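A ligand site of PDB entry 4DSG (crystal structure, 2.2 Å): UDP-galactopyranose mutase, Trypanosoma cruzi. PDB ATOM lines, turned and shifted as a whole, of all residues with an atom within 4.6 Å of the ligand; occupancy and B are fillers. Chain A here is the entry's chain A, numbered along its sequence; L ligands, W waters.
An oxygen (O7) of the ligand lies within hydrogen-bond range of the side-chain hydroxyl of Tyr 320 (2.6 Å).
OD1 of Asn 160 sits at hydrogen-bond distance from O3 of the ligand.
An oxygen (O11) of the ligand lies within salt-bridge range of the guanidinium group of Arg 330.
OH of Tyr 432 sits at hydrogen-bond distance from O12 of the ligand.
OH of Tyr 398 is in hydrogen-bond range of O10 of the ligand, at 2.8 Å.
N2 of the ligand is in hydrogen-bond range of OE1 of Gln 106 (2.8 Å).
The backbone NH (N) of Phe 105 lies within hydrogen-bond range of an oxygen (O2) of the ligand.
The guanidinium group (NH1) of Arg 179 lies within salt-bridge range of an oxygen (O12) of the ligand, at 3.5 Å.
NE1 of Trp 164 sits at hydrogen-bond distance from O5 of the ligand (3.1 Å).
OD1 of Asn 160 lies within hydrogen-bond range of NE1 of Trp 164.
The side-chain amide nitrogen (ND2) of Asn 160 lies within hydrogen-bond range of the backbone carbonyl oxygen (O) of Met 156 (2.8 Å).
The guanidinium group (NH2) of Arg 330 sits at hydrogen-bond distance from the side-chain hydroxyl (OH) of Tyr 398, 3.3 Å away.
The side-chain hydroxyl of Tyr 432 sits at hydrogen-bond distance from the guanidinium group of Arg 179 (3.1 Å).
NE2 of Gln 106 sits at hydrogen-bond distance from O of Ala 181, 2.9 Å away.
Tyr 103 touches the ligand.
Pro 104 touches the ligand.
CZ of Phe 139 touches O3 of the ligand (3.99 Å).
Phe 155 touches the ligand (CZ to C2, 3.4 Å).
CE of Met 156 touches O1 of the ligand, at 3.4 Å.
Val 180 touches the ligand (CG1 to O1, 3.8 Å).
Hydrophobic or aromatic side chains within 4 Å of the ligand: Tyr 103, Phe 105, Phe 139, Phe 155, Met 156, Trp 164, Val 180, Tyr 320, Tyr 398 and Tyr 432.
Water W1 lies within hydrogen-bond range of OH of Tyr 103, O8 of the ligand and O of Arg 179.
Water W3 lies within hydrogen-bond range of an oxygen (O8) of the ligand and the guanidinium group of Arg 179.
Water W7 bridges the side-chain hydroxyl of Tyr 159 (2.6 Å) and an oxygen (O7) of the ligand (2.7 Å).
Water W2 lies within hydrogen-bond range of an oxygen (O8) of the ligand (3.0 Å) and the side-chain hydroxyl (OH) of Tyr 320 (3.1 Å).
Water W4 lies within hydrogen-bond range of O of Arg 179 (2.7 Å), N of Ala 181 (3.0 Å), O1 of the ligand (3.4 Å) and OH of Tyr 103 (3.4 Å).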
ATOM      1  N   VAL A  94       3.397  12.366  19.633  1.00  0.00           N
ATOM      2  CA  VAL A  94       4.110  13.641  19.611  1.00  0.00           C
ATOM      3  C   VAL A  94       5.262  13.570  18.604  1.00  0.00           C
ATOM      4  O   VAL A  94       6.118  12.676  18.673  1.00  0.00           O
ATOM      5  CB  VAL A  94       4.679  13.989  21.018  1.00  0.00           C
ATOM      6  CG1 VAL A  94       5.321  15.374  21.003  1.00  0.00           C
ATOM      7  CG2 VAL A  94       3.601  13.926  22.074  1.00  0.00           C
ATOM      8  N   TYR A 103       1.778   9.592  23.246  1.00  0.00           N
ATOM      9  CA  TYR A 103       1.236  10.479  24.280  1.00  0.00           C
ATOM     10  C   TYR A 103       1.019   9.676  25.558  1.00  0.00           C
ATOM     11  O   TYR A 103       0.657   8.501  25.508  1.00  0.00           O
ATOM     12  CB  TYR A 103      -0.120  11.041  23.798  1.00  0.00           C
ATOM     13  CG  TYR A 103      -0.948  11.682  24.903  1.00  0.00           C
ATOM     14  CD1 TYR A 103      -1.792  10.907  25.688  1.00  0.00           C
ATOM     15  CD2 TYR A 103      -0.888  13.054  25.160  1.00  0.00           C
ATOM     16  CE1 TYR A 103      -2.553  11.474  26.705  1.00  0.00           C
ATOM     17  CE2 TYR A 103      -1.629  13.627  26.167  1.00  0.00           C
ATOM     18  CZ  TYR A 103      -2.461  12.835  26.944  1.00  0.00           C
ATOM     19  OH  TYR A 103      -3.232  13.404  27.951  1.00  0.00           O
ATOM     20  N   PRO A 104       1.248  10.300  26.727  1.00  0.00           N
ATOM     21  CA  PRO A 104       1.836  11.614  26.990  1.00  0.00           C
ATOM     22  C   PRO A 104       3.352  11.541  26.835  1.00  0.00           C
ATOM     23  O   PRO A 104       3.979  10.536  27.183  1.00  0.00           O
ATOM     24  CB  PRO A 104       1.511  11.871  28.474  1.00  0.00           C
ATOM     25  CG  PRO A 104       0.485  10.801  28.859  1.00  0.00           C
ATOM     26  CD  PRO A 104       0.825   9.641  27.978  1.00  0.00           C
ATOM     27  N   PHE A 105       3.922  12.632  26.317  1.00  0.00           N
ATOM     28  CA  PHE A 105       5.351  12.716  26.081  1.00  0.00           C
ATOM     29  C   PHE A 105       6.171  12.287  27.297  1.00  0.00           C
ATOM     30  O   PHE A 105       7.081  11.455  27.184  1.00  0.00           O
ATOM     31  CB  PHE A 105       5.725  14.152  25.708  1.00  0.00           C
ATOM     32  CG  PHE A 105       7.201  14.359  25.577  1.00  0.00           C
ATOM     33  CD1 PHE A 105       7.835  14.138  24.366  1.00  0.00           C
ATOM     34  CD2 PHE A 105       7.960  14.718  26.675  1.00  0.00           C
ATOM     35  CE1 PHE A 105       9.205  14.304  24.255  1.00  0.00           C
ATOM     36  CE2 PHE A 105       9.329  14.890  26.577  1.00  0.00           C
ATOM     37  CZ  PHE A 105       9.952  14.680  25.361  1.00  0.00           C
ATOM     38  N   GLN A 106       5.841  12.870  28.453  1.00  0.00           N
ATOM     39  CA  GLN A 106       6.652  12.727  29.661  1.00  0.00           C
ATOM     40  C   GLN A 106       6.711  11.285  30.153  1.00  0.00           C
ATOM     41  O   GLN A 106       7.666  10.900  30.816  1.00  0.00           O
ATOM     42  CB  GLN A 106       6.127  13.635  30.780  1.00  0.00           C
ATOM     43  CG  GLN A 106       4.666  13.383  31.196  1.00  0.00           C
ATOM     44  CD  GLN A 106       3.690  14.265  30.441  1.00  0.00           C
ATOM     45  OE1 GLN A 106       3.791  14.429  29.222  1.00  0.00           O
ATOM     46  NE2 GLN A 106       2.746  14.849  31.169  1.00  0.00           N
ATOM     47  N   PHE A 139       2.865  27.611  36.456  1.00  0.00           N
ATOM     48  CA  PHE A 139       2.872  26.368  35.686  1.00  0.00           C
ATOM     49  C   PHE A 139       4.280  25.965  35.232  1.00  0.00           C
ATOM     50  O   PHE A 139       4.681  24.809  35.395  1.00  0.00           O
ATOM     51  CB  PHE A 139       1.864  26.471  34.524  1.00  0.00           C
ATOM     52  CG  PHE A 139       1.733  25.193  33.702  1.00  0.00           C
ATOM     53  CD1 PHE A 139       1.621  23.952  34.320  1.00  0.00           C
ATOM     54  CD2 PHE A 139       1.705  25.257  32.305  1.00  0.00           C
ATOM     55  CE1 PHE A 139       1.498  22.792  33.559  1.00  0.00           C
ATOM     56  CE2 PHE A 139       1.593  24.088  31.539  1.00  0.00           C
ATOM     57  CZ  PHE A 139       1.480  22.852  32.171  1.00  0.00           C
ATOM     58  N   PHE A 155      10.002  19.371  25.554  1.00  0.00           N
ATOM     59  CA  PHE A 155       8.565  19.358  25.319  1.00  0.00           C
ATOM     60  C   PHE A 155       7.732  20.436  26.046  1.00  0.00           C
ATOM     61  O   PHE A 155       7.048  21.210  25.406  1.00  0.00           O
ATOM     62  CB  PHE A 155       7.964  17.980  25.607  1.00  0.00           C
ATOM     63  CG  PHE A 155       6.481  17.927  25.402  1.00  0.00           C
ATOM     64  CD1 PHE A 155       5.955  17.744  24.129  1.00  0.00           C
ATOM     65  CD2 PHE A 155       5.608  18.128  26.453  1.00  0.00           C
ATOM     66  CE1 PHE A 155       4.579  17.729  23.913  1.00  0.00           C
ATOM     67  CE2 PHE A 155       4.222  18.108  26.246  1.00  0.00           C
ATOM     68  CZ  PHE A 155       3.717  17.914  24.978  1.00  0.00           C
ATOM     69  N   MET A 156       7.809  20.481  27.378  1.00  0.00           N
ATOM     70  CA  MET A 156       6.846  21.256  28.144  1.00  0.00           C
ATOM     71  C   MET A 156       6.864  22.733  27.816  1.00  0.00           C
ATOM     72  O   MET A 156       5.806  23.341  27.601  1.00  0.00           O
ATOM     73  CB  MET A 156       7.060  21.055  29.649  1.00  0.00           C
ATOM     74  CG  MET A 156       6.597  19.699  30.147  1.00  0.00           C
ATOM     75  SD  MET A 156       4.804  19.437  29.975  1.00  0.00           S
ATOM     76  CE  MET A 156       4.680  17.729  30.481  1.00  0.00           C
ATOM     77  N   TYR A 159       6.110  23.265  23.844  1.00  0.00           N
ATOM     78  CA  TYR A 159       4.743  22.868  23.476  1.00  0.00           C
ATOM     79  C   TYR A 159       3.715  23.778  24.140  1.00  0.00           C
ATOM     80  O   TYR A 159       2.752  24.231  23.495  1.00  0.00           O
ATOM     81  CB  TYR A 159       4.392  21.394  23.766  1.00  0.00           C
ATOM     82  CG  TYR A 159       2.969  21.147  23.290  1.00  0.00           C
ATOM     83  CD1 TYR A 159       2.690  21.008  21.949  1.00  0.00           C
ATOM     84  CD2 TYR A 159       1.902  21.176  24.189  1.00  0.00           C
ATOM     85  CE1 TYR A 159       1.388  20.861  21.499  1.00  0.00           C
ATOM     86  CE2 TYR A 159       0.601  21.020  23.757  1.00  0.00           C
ATOM     87  CZ  TYR A 159       0.353  20.866  22.408  1.00  0.00           C
ATOM     88  OH  TYR A 159      -0.930  20.730  21.962  1.00  0.00           O
ATOM     89  N   ASN A 160       3.898  24.066  25.418  1.00  0.00           N
ATOM     90  CA  ASN A 160       2.919  24.896  26.100  1.00  0.00           C
ATOM     91  C   ASN A 160       2.792  26.320  25.560  1.00  0.00           C
ATOM     92  O   ASN A 160       1.675  26.811  25.374  1.00  0.00           O
ATOM     93  CB  ASN A 160       3.098  24.842  27.614  1.00  0.00           C
ATOM     94  CG  ASN A 160       2.452  23.608  28.216  1.00  0.00           C
ATOM     95  OD1 ASN A 160       1.236  23.502  28.248  1.00  0.00           O
ATOM     96  ND2 ASN A 160       3.265  22.646  28.661  1.00  0.00           N
ATOM     97  N   VAL A 163       0.767  26.015  22.235  1.00  0.00           N
ATOM     98  CA  VAL A 163      -0.685  25.862  22.269  1.00  0.00           C
ATOM     99  C   VAL A 163      -1.378  27.043  22.968  1.00  0.00           C
ATOM    100  O   VAL A 163      -2.342  27.602  22.434  1.00  0.00           O
ATOM    101  CB  VAL A 163      -1.147  24.508  22.866  1.00  0.00           C
ATOM    102  CG1 VAL A 163      -0.591  24.295  24.251  1.00  0.00           C
ATOM    103  CG2 VAL A 163      -2.698  24.434  22.872  1.00  0.00           C
ATOM    104  N   TRP A 164      -0.865  27.439  24.125  1.00  0.00           N
ATOM    105  CA  TRP A 164      -1.523  28.472  24.922  1.00  0.00           C
ATOM    106  C   TRP A 164      -1.317  29.880  24.393  1.00  0.00           C
ATOM    107  O   TRP A 164      -2.111  30.757  24.683  1.00  0.00           O
ATOM    108  CB  TRP A 164      -1.081  28.404  26.375  1.00  0.00           C
ATOM    109  CG  TRP A 164      -1.525  27.162  27.095  1.00  0.00           C
ATOM    110  CD1 TRP A 164      -0.770  26.082  27.394  1.00  0.00           C
ATOM    111  CD2 TRP A 164      -2.843  26.885  27.602  1.00  0.00           C
ATOM    112  NE1 TRP A 164      -1.516  25.139  28.059  1.00  0.00           N
ATOM    113  CE2 TRP A 164      -2.802  25.614  28.201  1.00  0.00           C
ATOM    114  CE3 TRP A 164      -4.052  27.589  27.610  1.00  0.00           C
ATOM    115  CZ2 TRP A 164      -3.916  25.021  28.804  1.00  0.00           C
ATOM    116  CZ3 TRP A 164      -5.166  27.000  28.203  1.00  0.00           C
ATOM    117  CH2 TRP A 164      -5.094  25.718  28.785  1.00  0.00           C
ATOM    118  N   TRP A 175      -5.137  23.632  37.364  1.00  0.00           N
ATOM    119  CA  TRP A 175      -6.081  23.209  36.345  1.00  0.00           C
ATOM    120  C   TRP A 175      -5.643  21.882  35.747  1.00  0.00           C
ATOM    121  O   TRP A 175      -6.313  21.351  34.866  1.00  0.00           O
ATOM    122  CB  TRP A 175      -6.119  24.247  35.222  1.00  0.00           C
ATOM    123  CG  TRP A 175      -4.742  24.533  34.683  1.00  0.00           C
ATOM    124  CD1 TRP A 175      -3.862  25.463  35.171  1.00  0.00           C
ATOM    125  CD2 TRP A 175      -4.062  23.874  33.609  1.00  0.00           C
ATOM    126  NE1 TRP A 175      -2.694  25.434  34.452  1.00  0.00           N
ATOM    127  CE2 TRP A 175      -2.786  24.462  33.487  1.00  0.00           C
ATOM    128  CE3 TRP A 175      -4.419  22.836  32.736  1.00  0.00           C
ATOM    129  CZ2 TRP A 175      -1.841  24.057  32.520  1.00  0.00           C
ATOM    130  CZ3 TRP A 175      -3.494  22.428  31.770  1.00  0.00           C
ATOM    131  CH2 TRP A 175      -2.209  23.037  31.677  1.00  0.00           C
ATOM    132  N   ARG A 179      -5.183  16.890  32.846  1.00  0.00           N
ATOM    133  CA  ARG A 179      -4.525  17.314  31.615  1.00  0.00           C
ATOM    134  C   ARG A 179      -3.031  16.965  31.561  1.00  0.00           C
ATOM    135  O   ARG A 179      -2.520  16.579  30.524  1.00  0.00           O
ATOM    136  CB  ARG A 179      -4.731  18.824  31.387  1.00  0.00           C
ATOM    137  CG  ARG A 179      -6.167  19.294  31.555  1.00  0.00           C
ATOM    138  CD  ARG A 179      -7.031  19.077  30.305  1.00  0.00           C
ATOM    139  NE  ARG A 179      -8.365  19.639  30.486  1.00  0.00           N
ATOM    140  CZ  ARG A 179      -9.220  19.921  29.502  1.00  0.00           C
ATOM    141  NH1 ARG A 179      -8.898  19.708  28.221  1.00  0.00           N
ATOM    142  NH2 ARG A 179     -10.409  20.441  29.789  1.00  0.00           N
ATOM    143  N   VAL A 180      -2.358  17.079  32.700  1.00  0.00           N
ATOM    144  CA  VAL A 180      -0.909  16.876  32.754  1.00  0.00           C
ATOM    145  C   VAL A 180      -0.570  15.644  33.585  1.00  0.00           C
ATOM    146  O   VAL A 180      -0.709  15.648  34.811  1.00  0.00           O
ATOM    147  CB  VAL A 180      -0.191  18.114  33.326  1.00  0.00           C
ATOM    148  CG1 VAL A 180       1.315  17.928  33.276  1.00  0.00           C
ATOM    149  CG2 VAL A 180      -0.592  19.360  32.548  1.00  0.00           C
ATOM    150  N   ALA A 181      -0.139  14.578  32.914  1.00  0.00           N
ATOM    151  CA  ALA A 181       0.093  13.306  33.558  1.00  0.00           C
ATOM    152  C   ALA A 181       1.388  13.343  34.364  1.00  0.00           C
ATOM    153  O   ALA A 181       2.384  13.915  33.909  1.00  0.00           O
ATOM    154  CB  ALA A 181       0.138  12.178  32.508  1.00  0.00           C
ATOM    155  N   TYR A 320       0.756  15.921  18.245  1.00  0.00           N
ATOM    156  CA  TYR A 320       1.298  17.113  18.881  1.00  0.00           C
ATOM    157  C   TYR A 320       2.629  17.548  18.266  1.00  0.00           C
ATOM    158  O   TYR A 320       3.460  16.699  17.921  1.00  0.00           O
ATOM    159  CB  TYR A 320       1.496  16.874  20.370  1.00  0.00           C
ATOM    160  CG  TYR A 320       0.235  16.632  21.140  1.00  0.00           C
ATOM    161  CD1 TYR A 320      -0.596  17.680  21.505  1.00  0.00           C
ATOM    162  CD2 TYR A 320      -0.124  15.343  21.531  1.00  0.00           C
ATOM    163  CE1 TYR A 320      -1.749  17.464  22.238  1.00  0.00           C
ATOM    164  CE2 TYR A 320      -1.286  15.117  22.260  1.00  0.00           C
ATOM    165  CZ  TYR A 320      -2.089  16.180  22.598  1.00  0.00           C
ATOM    166  OH  TYR A 320      -3.243  15.978  23.326  1.00  0.00           O
ATOM    167  N   ARG A 330      -1.195  21.277  17.082  1.00  0.00           N
ATOM    168  CA  ARG A 330      -1.834  19.963  16.932  1.00  0.00           C
ATOM    169  C   ARG A 330      -2.347  19.755  15.517  1.00  0.00           C
ATOM    170  O   ARG A 330      -2.779  20.717  14.859  1.00  0.00           O
ATOM    171  CB  ARG A 330      -2.984  19.822  17.925  1.00  0.00           C
ATOM    172  CG  ARG A 330      -3.764  18.510  17.814  1.00  0.00           C
ATOM    173  CD  ARG A 330      -4.593  18.283  19.082  1.00  0.00           C
ATOM    174  NE  ARG A 330      -5.491  19.394  19.336  1.00  0.00           N
ATOM    175  CZ  ARG A 330      -5.976  19.729  20.524  1.00  0.00           C
ATOM    176  NH1 ARG A 330      -5.633  19.044  21.609  1.00  0.00           N
ATOM    177  NH2 ARG A 330      -6.797  20.767  20.634  1.00  0.00           N
ATOM    178  N   TYR A 398      -9.287  29.557  23.758  1.00  0.00           N
ATOM    179  CA  TYR A 398      -8.998  28.923  25.041  1.00  0.00           C
ATOM    180  C   TYR A 398      -9.095  29.977  26.126  1.00  0.00           C
ATOM    181  O   TYR A 398      -8.533  31.053  25.972  1.00  0.00           O
ATOM    182  CB  TYR A 398      -7.577  28.397  25.078  1.00  0.00           C
ATOM    183  CG  TYR A 398      -7.330  27.068  24.413  1.00  0.00           C
ATOM    184  CD1 TYR A 398      -6.856  25.984  25.137  1.00  0.00           C
ATOM    185  CD2 TYR A 398      -7.537  26.907  23.037  1.00  0.00           C
ATOM    186  CE1 TYR A 398      -6.599  24.754  24.524  1.00  0.00           C
ATOM    187  CE2 TYR A 398      -7.282  25.694  22.410  1.00  0.00           C
ATOM    188  CZ  TYR A 398      -6.809  24.630  23.164  1.00  0.00           C
ATOM    189  OH  TYR A 398      -6.556  23.430  22.532  1.00  0.00           O
ATOM    190  N   TYR A 432     -11.093  26.720  32.162  1.00  0.00           N
ATOM    191  CA  TYR A 432     -10.550  25.731  31.236  1.00  0.00           C
ATOM    192  C   TYR A 432     -10.702  24.284  31.714  1.00  0.00           C
ATOM    193  O   TYR A 432     -11.086  23.416  30.948  1.00  0.00           O
ATOM    194  CB  TYR A 432      -9.061  26.004  30.958  1.00  0.00           C
ATOM    195  CG  TYR A 432      -8.392  24.870  30.194  1.00  0.00           C
ATOM    196  CD1 TYR A 432      -8.570  24.726  28.813  1.00  0.00           C
ATOM    197  CD2 TYR A 432      -7.611  23.932  30.857  1.00  0.00           C
ATOM    198  CE1 TYR A 432      -7.981  23.683  28.124  1.00  0.00           C
ATOM    199  CE2 TYR A 432      -7.002  22.891  30.168  1.00  0.00           C
ATOM    200  CZ  TYR A 432      -7.193  22.778  28.812  1.00  0.00           C
ATOM    201  OH  TYR A 432      -6.585  21.743  28.136  1.00  0.00           O
HETATM  202  N1  LIG L   1       0.260  17.751  27.732  1.00  0.00           N
HETATM  203  C1  LIG L   1       1.231  16.927  28.402  1.00  0.00           C
HETATM  204  N2  LIG L   1       1.873  15.857  27.688  1.00  0.00           N
HETATM  205  C2  LIG L   1       1.543  15.626  26.343  1.00  0.00           C
HETATM  206  C3  LIG L   1       0.538  16.487  25.656  1.00  0.00           C
HETATM  207  C4  LIG L   1      -0.079  17.509  26.360  1.00  0.00           C
HETATM  208  O1  LIG L   1       1.454  17.114  29.593  1.00  0.00           O
HETATM  209  O2  LIG L   1       2.087  14.727  25.716  1.00  0.00           O
HETATM  210  C5  LIG L   1      -0.383  18.830  28.450  1.00  0.00           C
HETATM  211  C6  LIG L   1      -0.100  20.174  27.835  1.00  0.00           C
HETATM  212  O3  LIG L   1       0.459  21.004  28.784  1.00  0.00           O
HETATM  213  C7  LIG L   1      -1.399  20.671  27.388  1.00  0.00           C
HETATM  214  C8  LIG L   1      -2.374  19.900  28.235  1.00  0.00           C
HETATM  215  O4  LIG L   1      -1.771  18.643  28.477  1.00  0.00           O
HETATM  216  O5  LIG L   1      -1.540  22.045  27.567  1.00  0.00           O
HETATM  217  C9  LIG L   1      -3.758  19.667  27.611  1.00  0.00           C
HETATM  218  O6  LIG L   1      -3.549  19.282  26.295  1.00  0.00           O
HETATM  219  P1  LIG L   1      -4.688  18.619  25.432  1.00  0.00           P
HETATM  220  O7  LIG L   1      -4.356  18.298  23.920  1.00  0.00           O
HETATM  221  O8  LIG L   1      -5.017  17.427  26.419  1.00  0.00           O
HETATM  222  O9  LIG L   1      -5.958  19.525  25.768  1.00  0.00           O
HETATM  223  P2  LIG L   1      -6.475  20.626  24.792  1.00  0.00           P
HETATM  224  O10 LIG L   1      -5.412  21.526  24.225  1.00  0.00           O
HETATM  225  O11 LIG L   1      -7.157  19.912  23.648  1.00  0.00           O
HETATM  226  O12 LIG L   1      -7.490  21.413  25.566  1.00  0.00           O
HETATM  227  O   HOH W   1      -3.283  16.043  27.882  1.00  0.00           O
HETATM  228  O   HOH W   2      -5.729  14.957  24.951  1.00  0.00           O
HETATM  229  O   HOH W   3      -7.557  17.119  27.339  1.00  0.00           O
HETATM  230  O   HOH W   4      -0.767  14.583  29.963  1.00  0.00           O
HETATM  231  O   HOH W   5      -3.755  22.833  26.078  1.00  0.00           O
HETATM  232  O   HOH W   6      -9.585  23.001  24.532  1.00  0.00           O
HETATM  233  O   HOH W   7      -2.841  20.564  23.719  1.00  0.00           O
